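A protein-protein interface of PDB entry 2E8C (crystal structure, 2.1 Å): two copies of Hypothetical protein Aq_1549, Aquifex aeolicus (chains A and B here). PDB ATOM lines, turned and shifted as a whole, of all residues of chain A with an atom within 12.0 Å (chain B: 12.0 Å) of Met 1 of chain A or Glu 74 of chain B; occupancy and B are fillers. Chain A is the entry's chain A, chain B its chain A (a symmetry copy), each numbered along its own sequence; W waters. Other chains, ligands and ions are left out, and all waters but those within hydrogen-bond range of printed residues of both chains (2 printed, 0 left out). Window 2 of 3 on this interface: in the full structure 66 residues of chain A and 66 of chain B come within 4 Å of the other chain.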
ATOM      1  N   MET A   1       6.281  -9.330  -6.155  1.00  0.00           N
ATOM      2  CA  MET A   1       7.406  -8.694  -5.417  1.00  0.00           C
ATOM      3  C   MET A   1       8.639  -9.575  -5.529  1.00  0.00           C
ATOM      4  O   MET A   1       8.690 -10.663  -4.950  1.00  0.00           O
ATOM      5  CB  MET A   1       7.042  -8.516  -3.941  1.00  0.00           C
ATOM      6  CG  MET A   1       5.821  -7.644  -3.710  1.00  0.00           C
ATOM      7  SD  MET A   1       4.394  -8.221  -4.660  1.00  0.00           S
ATOM      8  CE  MET A   1       3.870  -9.606  -3.655  1.00  0.00           C
ATOM      9  N   GLU A   2       9.628  -9.118  -6.289  1.00  0.00           N
ATOM     10  CA  GLU A   2      10.844  -9.894  -6.437  1.00  0.00           C
ATOM     11  C   GLU A   2      11.556  -9.937  -5.099  1.00  0.00           C
ATOM     12  O   GLU A   2      11.635  -8.936  -4.387  1.00  0.00           O
ATOM     13  CB  GLU A   2      11.776  -9.289  -7.487  1.00  0.00           C
ATOM     14  CG  GLU A   2      13.149  -9.948  -7.469  1.00  0.00           C
ATOM     15  CD  GLU A   2      14.086  -9.430  -8.534  1.00  0.00           C
ATOM     16  OE1 GLU A   2      14.195  -8.195  -8.684  1.00  0.00           O
ATOM     17  OE2 GLU A   2      14.726 -10.266  -9.209  1.00  0.00           O
ATOM     18  N   VAL A   3      12.067 -11.111  -4.763  1.00  0.00           N
ATOM     19  CA  VAL A   3      12.780 -11.299  -3.514  1.00  0.00           C
ATOM     20  C   VAL A   3      14.272 -11.437  -3.764  1.00  0.00           C
ATOM     21  O   VAL A   3      14.694 -12.208  -4.629  1.00  0.00           O
ATOM     22  CB  VAL A   3      12.282 -12.564  -2.781  1.00  0.00           C
ATOM     23  CG1 VAL A   3      13.174 -12.865  -1.586  1.00  0.00           C
ATOM     24  CG2 VAL A   3      10.847 -12.369  -2.329  1.00  0.00           C
ATOM     25  N   LYS A   4      15.066 -10.674  -3.016  1.00  0.00           N
ATOM     26  CA  LYS A   4      16.519 -10.735  -3.113  1.00  0.00           C
ATOM     27  C   LYS A   4      17.003 -11.260  -1.761  1.00  0.00           C
ATOM     28  O   LYS A   4      16.490 -10.856  -0.709  1.00  0.00           O
ATOM     29  CB  LYS A   4      17.123  -9.351  -3.365  1.00  0.00           C
ATOM     30  CG  LYS A   4      16.767  -8.712  -4.701  1.00  0.00           C
ATOM     31  CD  LYS A   4      17.390  -9.445  -5.881  1.00  0.00           C
ATOM     32  CE  LYS A   4      17.240  -8.625  -7.159  1.00  0.00           C
ATOM     33  NZ  LYS A   4      17.787  -9.334  -8.340  1.00  0.00           N
ATOM     34  N   GLU A   5      17.974 -12.165  -1.785  1.00  0.00           N
ATOM     35  CA  GLU A   5      18.501 -12.735  -0.554  1.00  0.00           C
ATOM     36  C   GLU A   5      20.010 -12.923  -0.569  1.00  0.00           C
ATOM     37  O   GLU A   5      20.588 -13.336  -1.571  1.00  0.00           O
ATOM     38  CB  GLU A   5      17.844 -14.085  -0.283  1.00  0.00           C
ATOM     39  CG  GLU A   5      16.460 -14.004   0.327  1.00  0.00           C
ATOM     40  CD  GLU A   5      15.884 -15.377   0.592  1.00  0.00           C
ATOM     41  OE1 GLU A   5      16.651 -16.259   1.028  1.00  0.00           O
ATOM     42  OE2 GLU A   5      14.671 -15.571   0.372  1.00  0.00           O
ATOM     43  N   LYS A 108      14.038   7.879 -11.562  1.00  0.00           N
ATOM     44  CA  LYS A 108      13.021   6.854 -11.756  1.00  0.00           C
ATOM     45  C   LYS A 108      13.443   5.391 -11.694  1.00  0.00           C
ATOM     46  O   LYS A 108      12.814   4.587 -11.010  1.00  0.00           O
ATOM     47  CB  LYS A 108      12.322   7.106 -13.093  1.00  0.00           C
ATOM     48  CG  LYS A 108      11.294   6.058 -13.486  1.00  0.00           C
ATOM     49  CD  LYS A 108      10.723   6.354 -14.867  1.00  0.00           C
ATOM     50  CE  LYS A 108       9.589   5.405 -15.224  1.00  0.00           C
ATOM     51  NZ  LYS A 108       8.450   5.541 -14.276  1.00  0.00           N
ATOM     52  N   TYR A 109      14.508   5.040 -12.400  1.00  0.00           N
ATOM     53  CA  TYR A 109      14.930   3.649 -12.465  1.00  0.00           C
ATOM     54  C   TYR A 109      15.849   3.016 -11.420  1.00  0.00           C
ATOM     55  O   TYR A 109      15.628   1.862 -11.048  1.00  0.00           O
ATOM     56  CB  TYR A 109      15.499   3.383 -13.857  1.00  0.00           C
ATOM     57  CG  TYR A 109      14.440   3.446 -14.939  1.00  0.00           C
ATOM     58  CD1 TYR A 109      13.429   2.488 -15.001  1.00  0.00           C
ATOM     59  CD2 TYR A 109      14.430   4.474 -15.882  1.00  0.00           C
ATOM     60  CE1 TYR A 109      12.435   2.549 -15.968  1.00  0.00           C
ATOM     61  CE2 TYR A 109      13.432   4.544 -16.863  1.00  0.00           C
ATOM     62  CZ  TYR A 109      12.439   3.574 -16.895  1.00  0.00           C
ATOM     63  OH  TYR A 109      11.450   3.614 -17.850  1.00  0.00           O
ATOM     64  N   CYS A 110      16.867   3.720 -10.932  1.00  0.00           N
ATOM     65  CA  CYS A 110      17.749   3.057  -9.979  1.00  0.00           C
ATOM     66  C   CYS A 110      17.177   2.912  -8.563  1.00  0.00           C
ATOM     67  O   CYS A 110      16.987   3.888  -7.825  1.00  0.00           O
ATOM     68  CB  CYS A 110      19.154   3.700  -9.956  1.00  0.00           C
ATOM     69  SG  CYS A 110      20.061   3.045  -8.525  1.00  0.00           S
ATOM     70  N   SER A 111      16.902   1.659  -8.211  1.00  0.00           N
ATOM     71  CA  SER A 111      16.334   1.279  -6.918  1.00  0.00           C
ATOM     72  C   SER A 111      17.200   1.594  -5.695  1.00  0.00           C
ATOM     73  O   SER A 111      16.693   2.070  -4.680  1.00  0.00           O
ATOM     74  CB  SER A 111      16.015  -0.218  -6.917  1.00  0.00           C
ATOM     75  OG  SER A 111      15.067  -0.548  -7.915  1.00  0.00           O
ATOM     76  N   ALA A 114      17.225   5.353  -4.979  1.00  0.00           N
ATOM     77  CA  ALA A 114      15.932   5.825  -4.495  1.00  0.00           C
ATOM     78  C   ALA A 114      15.797   5.588  -2.995  1.00  0.00           C
ATOM     79  O   ALA A 114      15.155   6.366  -2.295  1.00  0.00           O
ATOM     80  CB  ALA A 114      14.801   5.119  -5.242  1.00  0.00           C
ATOM     81  N   MET A 115      16.424   4.524  -2.497  1.00  0.00           N
ATOM     82  CA  MET A 115      16.341   4.203  -1.077  1.00  0.00           C
ATOM     83  C   MET A 115      17.159   5.098  -0.148  1.00  0.00           C
ATOM     84  O   MET A 115      16.816   5.235   1.024  1.00  0.00           O
ATOM     85  CB  MET A 115      16.716   2.739  -0.834  1.00  0.00           C
ATOM     86  CG  MET A 115      15.671   1.753  -1.352  1.00  0.00           C
ATOM     87  SD  MET A 115      15.962   0.051  -0.838  1.00  0.00           S
ATOM     88  CE  MET A 115      15.348   0.137   0.801  1.00  0.00           C
ATOM     89  N   MET B  35      21.317  -4.621  -6.234  1.00  0.00           N
ATOM     90  CA  MET B  35      20.423  -4.669  -5.079  1.00  0.00           C
ATOM     91  C   MET B  35      20.831  -5.743  -4.064  1.00  0.00           C
ATOM     92  O   MET B  35      20.522  -5.623  -2.882  1.00  0.00           O
ATOM     93  CB  MET B  35      18.972  -4.855  -5.537  1.00  0.00           C
ATOM     94  CG  MET B  35      18.311  -3.530  -5.993  1.00  0.00           C
ATOM     95  SD  MET B  35      17.951  -2.364  -4.608  1.00  0.00           S
ATOM     96  CE  MET B  35      16.243  -2.836  -4.244  1.00  0.00           C
ATOM     97  N   LEU B  39      22.179  -5.166   0.118  1.00  0.00           N
ATOM     98  CA  LEU B  39      21.925  -6.023   1.275  1.00  0.00           C
ATOM     99  C   LEU B  39      23.236  -6.455   1.929  1.00  0.00           C
ATOM    100  O   LEU B  39      23.325  -6.550   3.156  1.00  0.00           O
ATOM    101  CB  LEU B  39      21.115  -7.255   0.861  1.00  0.00           C
ATOM    102  CG  LEU B  39      19.668  -6.985   0.433  1.00  0.00           C
ATOM    103  CD1 LEU B  39      18.995  -8.292   0.064  1.00  0.00           C
ATOM    104  CD2 LEU B  39      18.908  -6.311   1.573  1.00  0.00           C
ATOM    105  N   LYS B  69      16.761 -10.676   3.642  1.00  0.00           N
ATOM    106  CA  LYS B  69      15.825 -10.912   2.557  1.00  0.00           C
ATOM    107  C   LYS B  69      15.099  -9.608   2.260  1.00  0.00           C
ATOM    108  O   LYS B  69      14.579  -8.958   3.168  1.00  0.00           O
ATOM    109  CB  LYS B  69      14.792 -11.981   2.932  1.00  0.00           C
ATOM    110  CG  LYS B  69      13.834 -12.257   1.783  1.00  0.00           C
ATOM    111  CD  LYS B  69      12.522 -12.889   2.216  1.00  0.00           C
ATOM    112  CE  LYS B  69      12.598 -14.398   2.278  1.00  0.00           C
ATOM    113  NZ  LYS B  69      11.222 -14.977   2.188  1.00  0.00           N
ATOM    114  N   GLY B  70      15.067  -9.227   0.991  1.00  0.00           N
ATOM    115  CA  GLY B  70      14.395  -8.000   0.614  1.00  0.00           C
ATOM    116  C   GLY B  70      13.283  -8.248  -0.385  1.00  0.00           C
ATOM    117  O   GLY B  70      13.453  -9.010  -1.342  1.00  0.00           O
ATOM    118  N   LYS B  71      12.141  -7.610  -0.151  1.00  0.00           N
ATOM    119  CA  LYS B  71      10.980  -7.733  -1.028  1.00  0.00           C
ATOM    120  C   LYS B  71      10.789  -6.402  -1.750  1.00  0.00           C
ATOM    121  O   LYS B  71      10.438  -5.391  -1.137  1.00  0.00           O
ATOM    122  CB  LYS B  71       9.734  -8.081  -0.209  1.00  0.00           C
ATOM    123  CG  LYS B  71       9.786  -9.462   0.436  1.00  0.00           C
ATOM    124  CD  LYS B  71       8.523  -9.741   1.237  1.00  0.00           C
ATOM    125  CE  LYS B  71       8.493 -11.168   1.775  1.00  0.00           C
ATOM    126  NZ  LYS B  71       9.697 -11.494   2.595  1.00  0.00           N
ATOM    127  N   ARG B  72      11.020  -6.423  -3.059  1.00  0.00           N
ATOM    128  CA  ARG B  72      10.941  -5.238  -3.902  1.00  0.00           C
ATOM    129  C   ARG B  72       9.563  -4.864  -4.430  1.00  0.00           C
ATOM    130  O   ARG B  72       8.739  -5.724  -4.740  1.00  0.00           O
ATOM    131  CB  ARG B  72      11.874  -5.405  -5.105  1.00  0.00           C
ATOM    132  CG  ARG B  72      13.288  -5.863  -4.766  1.00  0.00           C
ATOM    133  CD  ARG B  72      14.115  -6.029  -6.033  1.00  0.00           C
ATOM    134  NE  ARG B  72      14.236  -4.777  -6.777  1.00  0.00           N
ATOM    135  CZ  ARG B  72      14.934  -4.638  -7.901  1.00  0.00           C
ATOM    136  NH1 ARG B  72      15.572  -5.679  -8.421  1.00  0.00           N
ATOM    137  NH2 ARG B  72      15.021  -3.453  -8.490  1.00  0.00           N
ATOM    138  N   ARG B  73       9.345  -3.558  -4.538  1.00  0.00           N
ATOM    139  CA  ARG B  73       8.112  -2.994  -5.065  1.00  0.00           C
ATOM    140  C   ARG B  73       8.064  -3.463  -6.517  1.00  0.00           C
ATOM    141  O   ARG B  73       9.103  -3.724  -7.124  1.00  0.00           O
ATOM    142  CB  ARG B  73       8.194  -1.463  -5.030  1.00  0.00           C
ATOM    143  CG  ARG B  73       6.931  -0.740  -5.444  1.00  0.00           C
ATOM    144  CD  ARG B  73       7.237   0.640  -6.016  1.00  0.00           C
ATOM    145  NE  ARG B  73       8.151   1.416  -5.184  1.00  0.00           N
ATOM    146  CZ  ARG B  73       8.644   2.605  -5.521  1.00  0.00           C
ATOM    147  NH1 ARG B  73       8.313   3.164  -6.674  1.00  0.00           N
ATOM    148  NH2 ARG B  73       9.482   3.235  -4.710  1.00  0.00           N
ATOM    149  N   GLU B  74       6.871  -3.560  -7.082  1.00  0.00           N
ATOM    150  CA  GLU B  74       6.747  -4.003  -8.461  1.00  0.00           C
ATOM    151  C   GLU B  74       6.949  -2.885  -9.484  1.00  0.00           C
ATOM    152  O   GLU B  74       7.350  -3.150 -10.614  1.00  0.00           O
ATOM    153  CB  GLU B  74       5.390  -4.689  -8.658  1.00  0.00           C
ATOM    154  CG  GLU B  74       5.301  -6.003  -7.883  1.00  0.00           C
ATOM    155  CD  GLU B  74       3.917  -6.623  -7.880  1.00  0.00           C
ATOM    156  OE1 GLU B  74       2.978  -6.016  -8.441  1.00  0.00           O
ATOM    157  OE2 GLU B  74       3.768  -7.726  -7.304  1.00  0.00           O
ATOM    158  N   LYS B  75       6.693  -1.638  -9.096  1.00  0.00           N
ATOM    159  CA  LYS B  75       6.874  -0.527 -10.028  1.00  0.00           C
ATOM    160  C   LYS B  75       8.149   0.270  -9.735  1.00  0.00           C
ATOM    161  O   LYS B  75       8.654   0.265  -8.610  1.00  0.00           O
ATOM    162  CB  LYS B  75       5.658   0.407 -10.003  1.00  0.00           C
ATOM    163  CG  LYS B  75       5.535   1.277  -8.765  1.00  0.00           C
ATOM    164  CD  LYS B  75       4.560   2.427  -9.005  1.00  0.00           C
ATOM    165  CE  LYS B  75       4.482   3.347  -7.802  1.00  0.00           C
ATOM    166  NZ  LYS B  75       5.829   3.846  -7.401  1.00  0.00           N
ATOM    167  N   HIS B  76       8.661   0.952 -10.756  1.00  0.00           N
ATOM    168  CA  HIS B  76       9.883   1.743 -10.629  1.00  0.00           C
ATOM    169  C   HIS B  76       9.740   3.002  -9.777  1.00  0.00           C
ATOM    170  O   HIS B  76       8.740   3.710  -9.863  1.00  0.00           O
ATOM    171  CB  HIS B  76      10.398   2.139 -12.013  1.00  0.00           C
ATOM    172  CG  HIS B  76      10.753   0.972 -12.878  1.00  0.00           C
ATOM    173  ND1 HIS B  76       9.919   0.497 -13.868  1.00  0.00           N
ATOM    174  CD2 HIS B  76      11.839   0.164 -12.883  1.00  0.00           C
ATOM    175  CE1 HIS B  76      10.479  -0.551 -14.445  1.00  0.00           C
ATOM    176  NE2 HIS B  76      11.644  -0.774 -13.864  1.00  0.00           N
ATOM    177  N   PRO B  77      10.743   3.282  -8.924  1.00  0.00           N
ATOM    178  CA  PRO B  77      11.932   2.433  -8.784  1.00  0.00           C
ATOM    179  C   PRO B  77      11.562   1.255  -7.890  1.00  0.00           C
ATOM    180  O   PRO B  77      10.828   1.417  -6.918  1.00  0.00           O
ATOM    181  CB  PRO B  77      12.952   3.369  -8.145  1.00  0.00           C
ATOM    182  CG  PRO B  77      12.091   4.241  -7.271  1.00  0.00           C
ATOM    183  CD  PRO B  77      10.898   4.537  -8.164  1.00  0.00           C
ATOM    184  N   LYS B  78      12.062   0.071  -8.223  1.00  0.00           N
ATOM    185  CA  LYS B  78      11.737  -1.123  -7.456  1.00  0.00           C
ATOM    186  C   LYS B  78      12.551  -1.286  -6.176  1.00  0.00           C
ATOM    187  O   LYS B  78      13.341  -2.227  -6.033  1.00  0.00           O
ATOM    188  CB  LYS B  78      11.876  -2.356  -8.355  1.00  0.00           C
ATOM    189  CG  LYS B  78      10.920  -2.329  -9.558  1.00  0.00           C
ATOM    190  CD  LYS B  78      11.078  -3.554 -10.464  1.00  0.00           C
ATOM    191  CE  LYS B  78      12.478  -3.618 -11.041  1.00  0.00           C
ATOM    192  NZ  LYS B  78      12.662  -4.742 -12.006  1.00  0.00           N
ATOM    193  N   ILE B  79      12.344  -0.364  -5.242  1.00  0.00           N
ATOM    194  CA  ILE B  79      13.038  -0.397  -3.964  1.00  0.00           C
ATOM    195  C   ILE B  79      12.501  -1.548  -3.122  1.00  0.00           C
ATOM    196  O   ILE B  79      11.505  -2.178  -3.473  1.00  0.00           O
ATOM    197  CB  ILE B  79      12.808   0.909  -3.181  1.00  0.00           C
ATOM    198  CG1 ILE B  79      11.318   1.047  -2.845  1.00  0.00           C
ATOM    199  CG2 ILE B  79      13.285   2.110  -4.005  1.00  0.00           C
ATOM    200  CD1 ILE B  79      10.978   2.264  -2.018  1.00  0.00           C
ATOM    201  N   TYR B  80      13.164  -1.832  -2.009  1.00  0.00           N
ATOM    202  CA  TYR B  80      12.684  -2.884  -1.124  1.00  0.00           C
ATOM    203  C   TYR B  80      11.562  -2.306  -0.265  1.00  0.00           C
ATOM    204  O   TYR B  80      11.784  -1.353   0.477  1.00  0.00           O
ATOM    205  CB  TYR B  80      13.793  -3.373  -0.193  1.00  0.00           C
ATOM    206  CG  TYR B  80      14.921  -4.120  -0.865  1.00  0.00           C
ATOM    207  CD1 TYR B  80      14.678  -5.266  -1.619  1.00  0.00           C
ATOM    208  CD2 TYR B  80      16.237  -3.693  -0.722  1.00  0.00           C
ATOM    209  CE1 TYR B  80      15.728  -5.972  -2.214  1.00  0.00           C
ATOM    210  CE2 TYR B  80      17.293  -4.389  -1.307  1.00  0.00           C
ATOM    211  CZ  TYR B  80      17.030  -5.527  -2.050  1.00  0.00           C
ATOM    212  OH  TYR B  80      18.075  -6.217  -2.618  1.00  0.00           O
ATOM    213  N   GLU B  81      10.363  -2.868  -0.371  1.00  0.00           N
ATOM    214  CA  GLU B  81       9.246  -2.412   0.449  1.00  0.00           C
ATOM    215  C   GLU B  81       9.481  -2.967   1.848  1.00  0.00           C
ATOM    216  O   GLU B  81       8.996  -2.423   2.844  1.00  0.00           O
ATOM    217  CB  GLU B  81       7.917  -2.957  -0.084  1.00  0.00           C
ATOM    218  CG  GLU B  81       7.501  -2.389  -1.426  1.00  0.00           C
ATOM    219  CD  GLU B  81       6.163  -2.929  -1.892  1.00  0.00           C
ATOM    220  OE1 GLU B  81       6.053  -4.160  -2.095  1.00  0.00           O
ATOM    221  OE2 GLU B  81       5.225  -2.120  -2.053  1.00  0.00           O
ATOM    222  N   GLU B  82      10.251  -4.048   1.911  1.00  0.00           N
ATOM    223  CA  GLU B  82      10.544  -4.696   3.175  1.00  0.00           C
ATOM    224  C   GLU B  82      11.917  -5.357   3.159  1.00  0.00           C
ATOM    225  O   GLU B  82      12.374  -5.846   2.123  1.00  0.00           O
ATOM    226  CB  GLU B  82       9.454  -5.739   3.467  1.00  0.00           C
ATOM    227  CG  GLU B  82       9.852  -6.868   4.409  1.00  0.00           C
ATOM    228  CD  GLU B  82       8.726  -7.877   4.623  1.00  0.00           C
ATOM    229  OE1 GLU B  82       7.537  -7.505   4.489  1.00  0.00           O
ATOM    230  OE2 GLU B  82       9.033  -9.044   4.934  1.00  0.00           O
ATOM    231  N   ILE B  83      12.580  -5.341   4.310  1.00  0.00           N
ATOM    232  CA  ILE B  83      13.890  -5.968   4.453  1.00  0.00           C
ATOM    233  C   ILE B  83      13.916  -6.741   5.762  1.00  0.00           C
ATOM    234  O   ILE B  83      13.766  -6.162   6.842  1.00  0.00           O
ATOM    235  CB  ILE B  83      15.041  -4.934   4.484  1.00  0.00           C
ATOM    236  CG1 ILE B  83      15.050  -4.113   3.193  1.00  0.00           C
ATOM    237  CG2 ILE B  83      16.385  -5.667   4.667  1.00  0.00           C
ATOM    238  CD1 ILE B  83      16.178  -3.102   3.115  1.00  0.00           C
ATOM    239  N   GLU B  84      14.094  -8.051   5.662  1.00  0.00           N
ATOM    240  CA  GLU B  84      14.157  -8.899   6.842  1.00  0.00           C
ATOM    241  C   GLU B  84      15.609  -9.213   7.143  1.00  0.00           C
ATOM    242  O   GLU B  84      16.344  -9.667   6.263  1.00  0.00           O
ATOM    243  CB  GLU B  84      13.423 -10.214   6.610  1.00  0.00           C
ATOM    244  CG  GLU B  84      11.932 -10.107   6.434  1.00  0.00           C
ATOM    245  CD  GLU B  84      11.310 -11.471   6.220  1.00  0.00           C
ATOM    246  OE1 GLU B  84      11.468 -12.338   7.108  1.00  0.00           O
ATOM    247  OE2 GLU B  84      10.679 -11.683   5.163  1.00  0.00           O
ATOM    248  N   SER B 119      13.005   4.564   4.115  1.00  0.00           N
ATOM    249  CA  SER B 119      12.350   4.185   2.869  1.00  0.00           C
ATOM    250  C   SER B 119      11.821   2.756   2.796  1.00  0.00           C
ATOM    251  O   SER B 119      11.339   2.342   1.744  1.00  0.00           O
ATOM    252  CB  SER B 119      13.305   4.412   1.693  1.00  0.00           C
ATOM    253  OG  SER B 119      13.604   5.786   1.528  1.00  0.00           O
ATOM    254  N   THR B 120      11.891   2.008   3.893  1.00  0.00           N
ATOM    255  CA  THR B 120      11.421   0.623   3.876  1.00  0.00           C
ATOM    256  C   THR B 120      10.895   0.159   5.234  1.00  0.00           C
ATOM    257  O   THR B 120      11.020   0.863   6.236  1.00  0.00           O
ATOM    258  CB  THR B 120      12.569  -0.328   3.441  1.00  0.00           C
ATOM    259  OG1 THR B 120      12.042  -1.624   3.133  1.00  0.00           O
ATOM    260  CG2 THR B 120      13.598  -0.464   4.553  1.00  0.00           C
ATOM    261  N   ASN B 121      10.292  -1.025   5.251  1.00  0.00           N
ATOM    262  CA  ASN B 121       9.784  -1.621   6.481  1.00  0.00           C
ATOM    263  C   ASN B 121      10.829  -2.649   6.914  1.00  0.00           C
ATOM    264  O   ASN B 121      11.056  -3.647   6.223  1.00  0.00           O
ATOM    265  CB  ASN B 121       8.434  -2.303   6.235  1.00  0.00           C
ATOM    266  CG  ASN B 121       7.980  -3.144   7.418  1.00  0.00           C
ATOM    267  OD1 ASN B 121       8.353  -2.882   8.561  1.00  0.00           O
ATOM    268  ND2 ASN B 121       7.156  -4.151   7.148  1.00  0.00           N
ATOM    269  N   LYS B 123      12.279  -5.560   9.358  1.00  0.00           N
ATOM    270  CA  LYS B 123      11.889  -6.599  10.299  1.00  0.00           C
ATOM    271  C   LYS B 123      13.152  -7.292  10.798  1.00  0.00           C
ATOM    272  O   LYS B 123      13.821  -8.012  10.055  1.00  0.00           O
ATOM    273  CB  LYS B 123      10.937  -7.596   9.630  1.00  0.00           C
ATOM    274  CG  LYS B 123       9.656  -6.925   9.133  1.00  0.00           C
ATOM    275  CD  LYS B 123       8.522  -7.913   8.896  1.00  0.00           C
ATOM    276  CE  LYS B 123       8.804  -8.850   7.739  1.00  0.00           C
ATOM    277  NZ  LYS B 123       7.637  -9.750   7.471  1.00  0.00           N
HETATM  278  O   HOH W   1      17.895  -6.775 -10.210  1.00  0.00           O
HETATM  279  O   HOH W   2      13.627  -0.042 -10.699  1.00  0.00           O
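Met 1 of chain A touches just these residues of chain B: Arg 72 (3.3 Å), Glu 74 (2.8 Å) and Glu 81 (3.8 Å).
Glu 74 of chain B touches just one residue of chain A: Met 1 (2.8 Å).
Val 3 of chain A touches just these residues of chain B: Lys 69 and Gly 70.
Of chain A, only Glu 2 (3.6 Å) comes within 4 Å of Lys 71 of chain B.
Of chain A, only Lys 108 (3.6 Å) and Tyr 109 (3.5 Å) come within 4 Å of His 76 of chain B.
Of chain A, only Ser 111 comes within 4 Å of Lys 78 of chain B.
Printed residues of chain A within 4 Å of Met 35 of chain B: Ser 111.
Of the printed residues of chain B, Lys 108 of chain A touches His 76 and Pro 77.
Printed residues of chain A within 4 Å of Lys 69 of chain B: Val 3, Lys 4 and Glu 5.
Printed residues of chain A within 4 Å of Gly 70 of chain B: Glu 2, Val 3 and Lys 4.
Asn 121 of chain B touches none of the printed residues of chain A.
Ile 83 of chain B touches none of the printed residues of chain A.
The nearest residue of chain A that does not touch Glu 74 of chain B is Glu 2 of chain A (5.6 Å).
The nearest printed residue of chain A that does not touch Ile 79 of chain B is Cys 110 of chain A (5.6 Å).
The side-chain amino group (NZ) of Lys 4 of chain A is in salt-bridge range of the side-chain carboxylate (OE2) of Glu 2 of chain A (3.3 Å).
The side-chain amino group of Lys 71 of chain B is in salt-bridge range of the side-chain carboxylate of Glu 84 of chain B, 2.8 Å away.
NE of Arg 72 of chain B lies within hydrogen-bond range of O of Lys 78 of chain B, at 2.8 Å.
The guanidinium group of Arg 73 of chain B lies close to the backbone carbonyl oxygen of Pro 77 of chain B, 3.1 Å away.
N of Arg 73 of chain B lies within hydrogen-bond range of O of Ile 79 of chain B (2.8 Å).
The side-chain hydroxyl of Thr 120 of chain B is in hydrogen-bond range of the backbone carbonyl oxygen of Tyr 80 of chain B (2.7 Å).
No position is printed for both chains.
Of the 28 pairs that touch across the chains among the printed residues, none has its exchanged pair printed and touching as well.
Water W2 lies within hydrogen-bond range of the backbone carbonyl oxygen of Tyr 109 of chain A, the backbone NH of Lys 78 of chain B and the side-chain hydroxyl of Ser 111 of chain A.
Water W1 lies within hydrogen-bond range of NH1 of Arg 72 of chain B and NZ of Lys 4 of chain A.
Among the printed residues, merely in contact across the chains: Val 3 of chain A with Gly 70 of chain B (3.2 Å), Met 1 of chain A with Arg 72 of chain B (3.3 Å), Lys 4 of chain A with Lys 69 of chain B (3.3 Å), Lys 4 of chain A with Tyr 80 of chain B (3.4 Å), Ser 111 of chain A with Ile 79 of chain B (3.5 Å), Val 3 of chain A with Lys 69 of chain B (3.5 Å), Ala 114 of chain A with Pro 77 of chain B (3.5 Å), Met 115 of chain A with Ile 79 of chain B (3.5 Å), Tyr 109 of chain A with His 76 of chain B (3.5 Å), Glu 2 of chain A with Gly 70 of chain B (3.5 Å), Lys 108 of chain A with His 76 of chain B (3.6 Å), Ala 114 of chain A with Ile 79 of chain B (3.6 Å), Lys 4 of chain A with Arg 72 of chain B (3.6 Å), Glu 2 of chain A with Lys 71 of chain B (3.6 Å), Lys 4 of chain A with Leu 39 of chain B (3.7 Å), Ser 111 of chain A with Met 35 of chain B (3.7 Å), Met 1 of chain A with Glu 81 of chain B (3.8 Å), Met 115 of chain A with Thr 120 of chain B (3.9 Å) and Ser 111 of chain A with Pro 77 of chain B (3.9 Å).
Of the 11 printed residues of chain A, 10 touch a printed residue of chain B.
Of the 22 printed residues of chain B, 15 touch a printed residue of chain A.
Hydrophobic or aromatic side chains of chain B within 4 Å of the printed part of chain A: Met 35, Leu 39, His 76, Pro 77, Ile 79 and Tyr 80.
Among the printed residues, 28 pairs touch across the chains.
The side-chain carboxylate (OE2) of Glu 74 of chain B is in hydrogen-bond range of the backbone NH (N) of Met 1 of chain A (3.2 Å).
OE1 of Glu 2 of chain A is in salt-bridge range of NH1 of Arg 72 of chain B (2.9 Å).
N of Gly 70 of chain B lies within hydrogen-bond range of O of Lys 4 of chain A, 2.8 Å away.
OE2 of Glu 5 of chain A is in salt-bridge range of NZ of Lys 69 of chain B (3.9 Å).
The guanidinium group (NH2) of Arg 72 of chain B lies within hydrogen-bond range of the side-chain hydroxyl (OG) of Ser 111 of chain A (3.0 Å).
OG of Ser 111 of chain A is in hydrogen-bond range of O of Lys 78 of chain B (3.1 Å).
The side-chain sulfur (SD) of Met 115 of chain A lies within hydrogen-bond range of the backbone NH (N) of Tyr 80 of chain B (3.6 Å).
OG of Ser 119 of chain B lies within hydrogen-bond range of O of Met 115 of chain A.
The backbone nitrogen (N) of Pro 77 of chain B lies close to the backbone carbonyl oxygen (O) of Lys 108 of chain A (3.2 Å).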
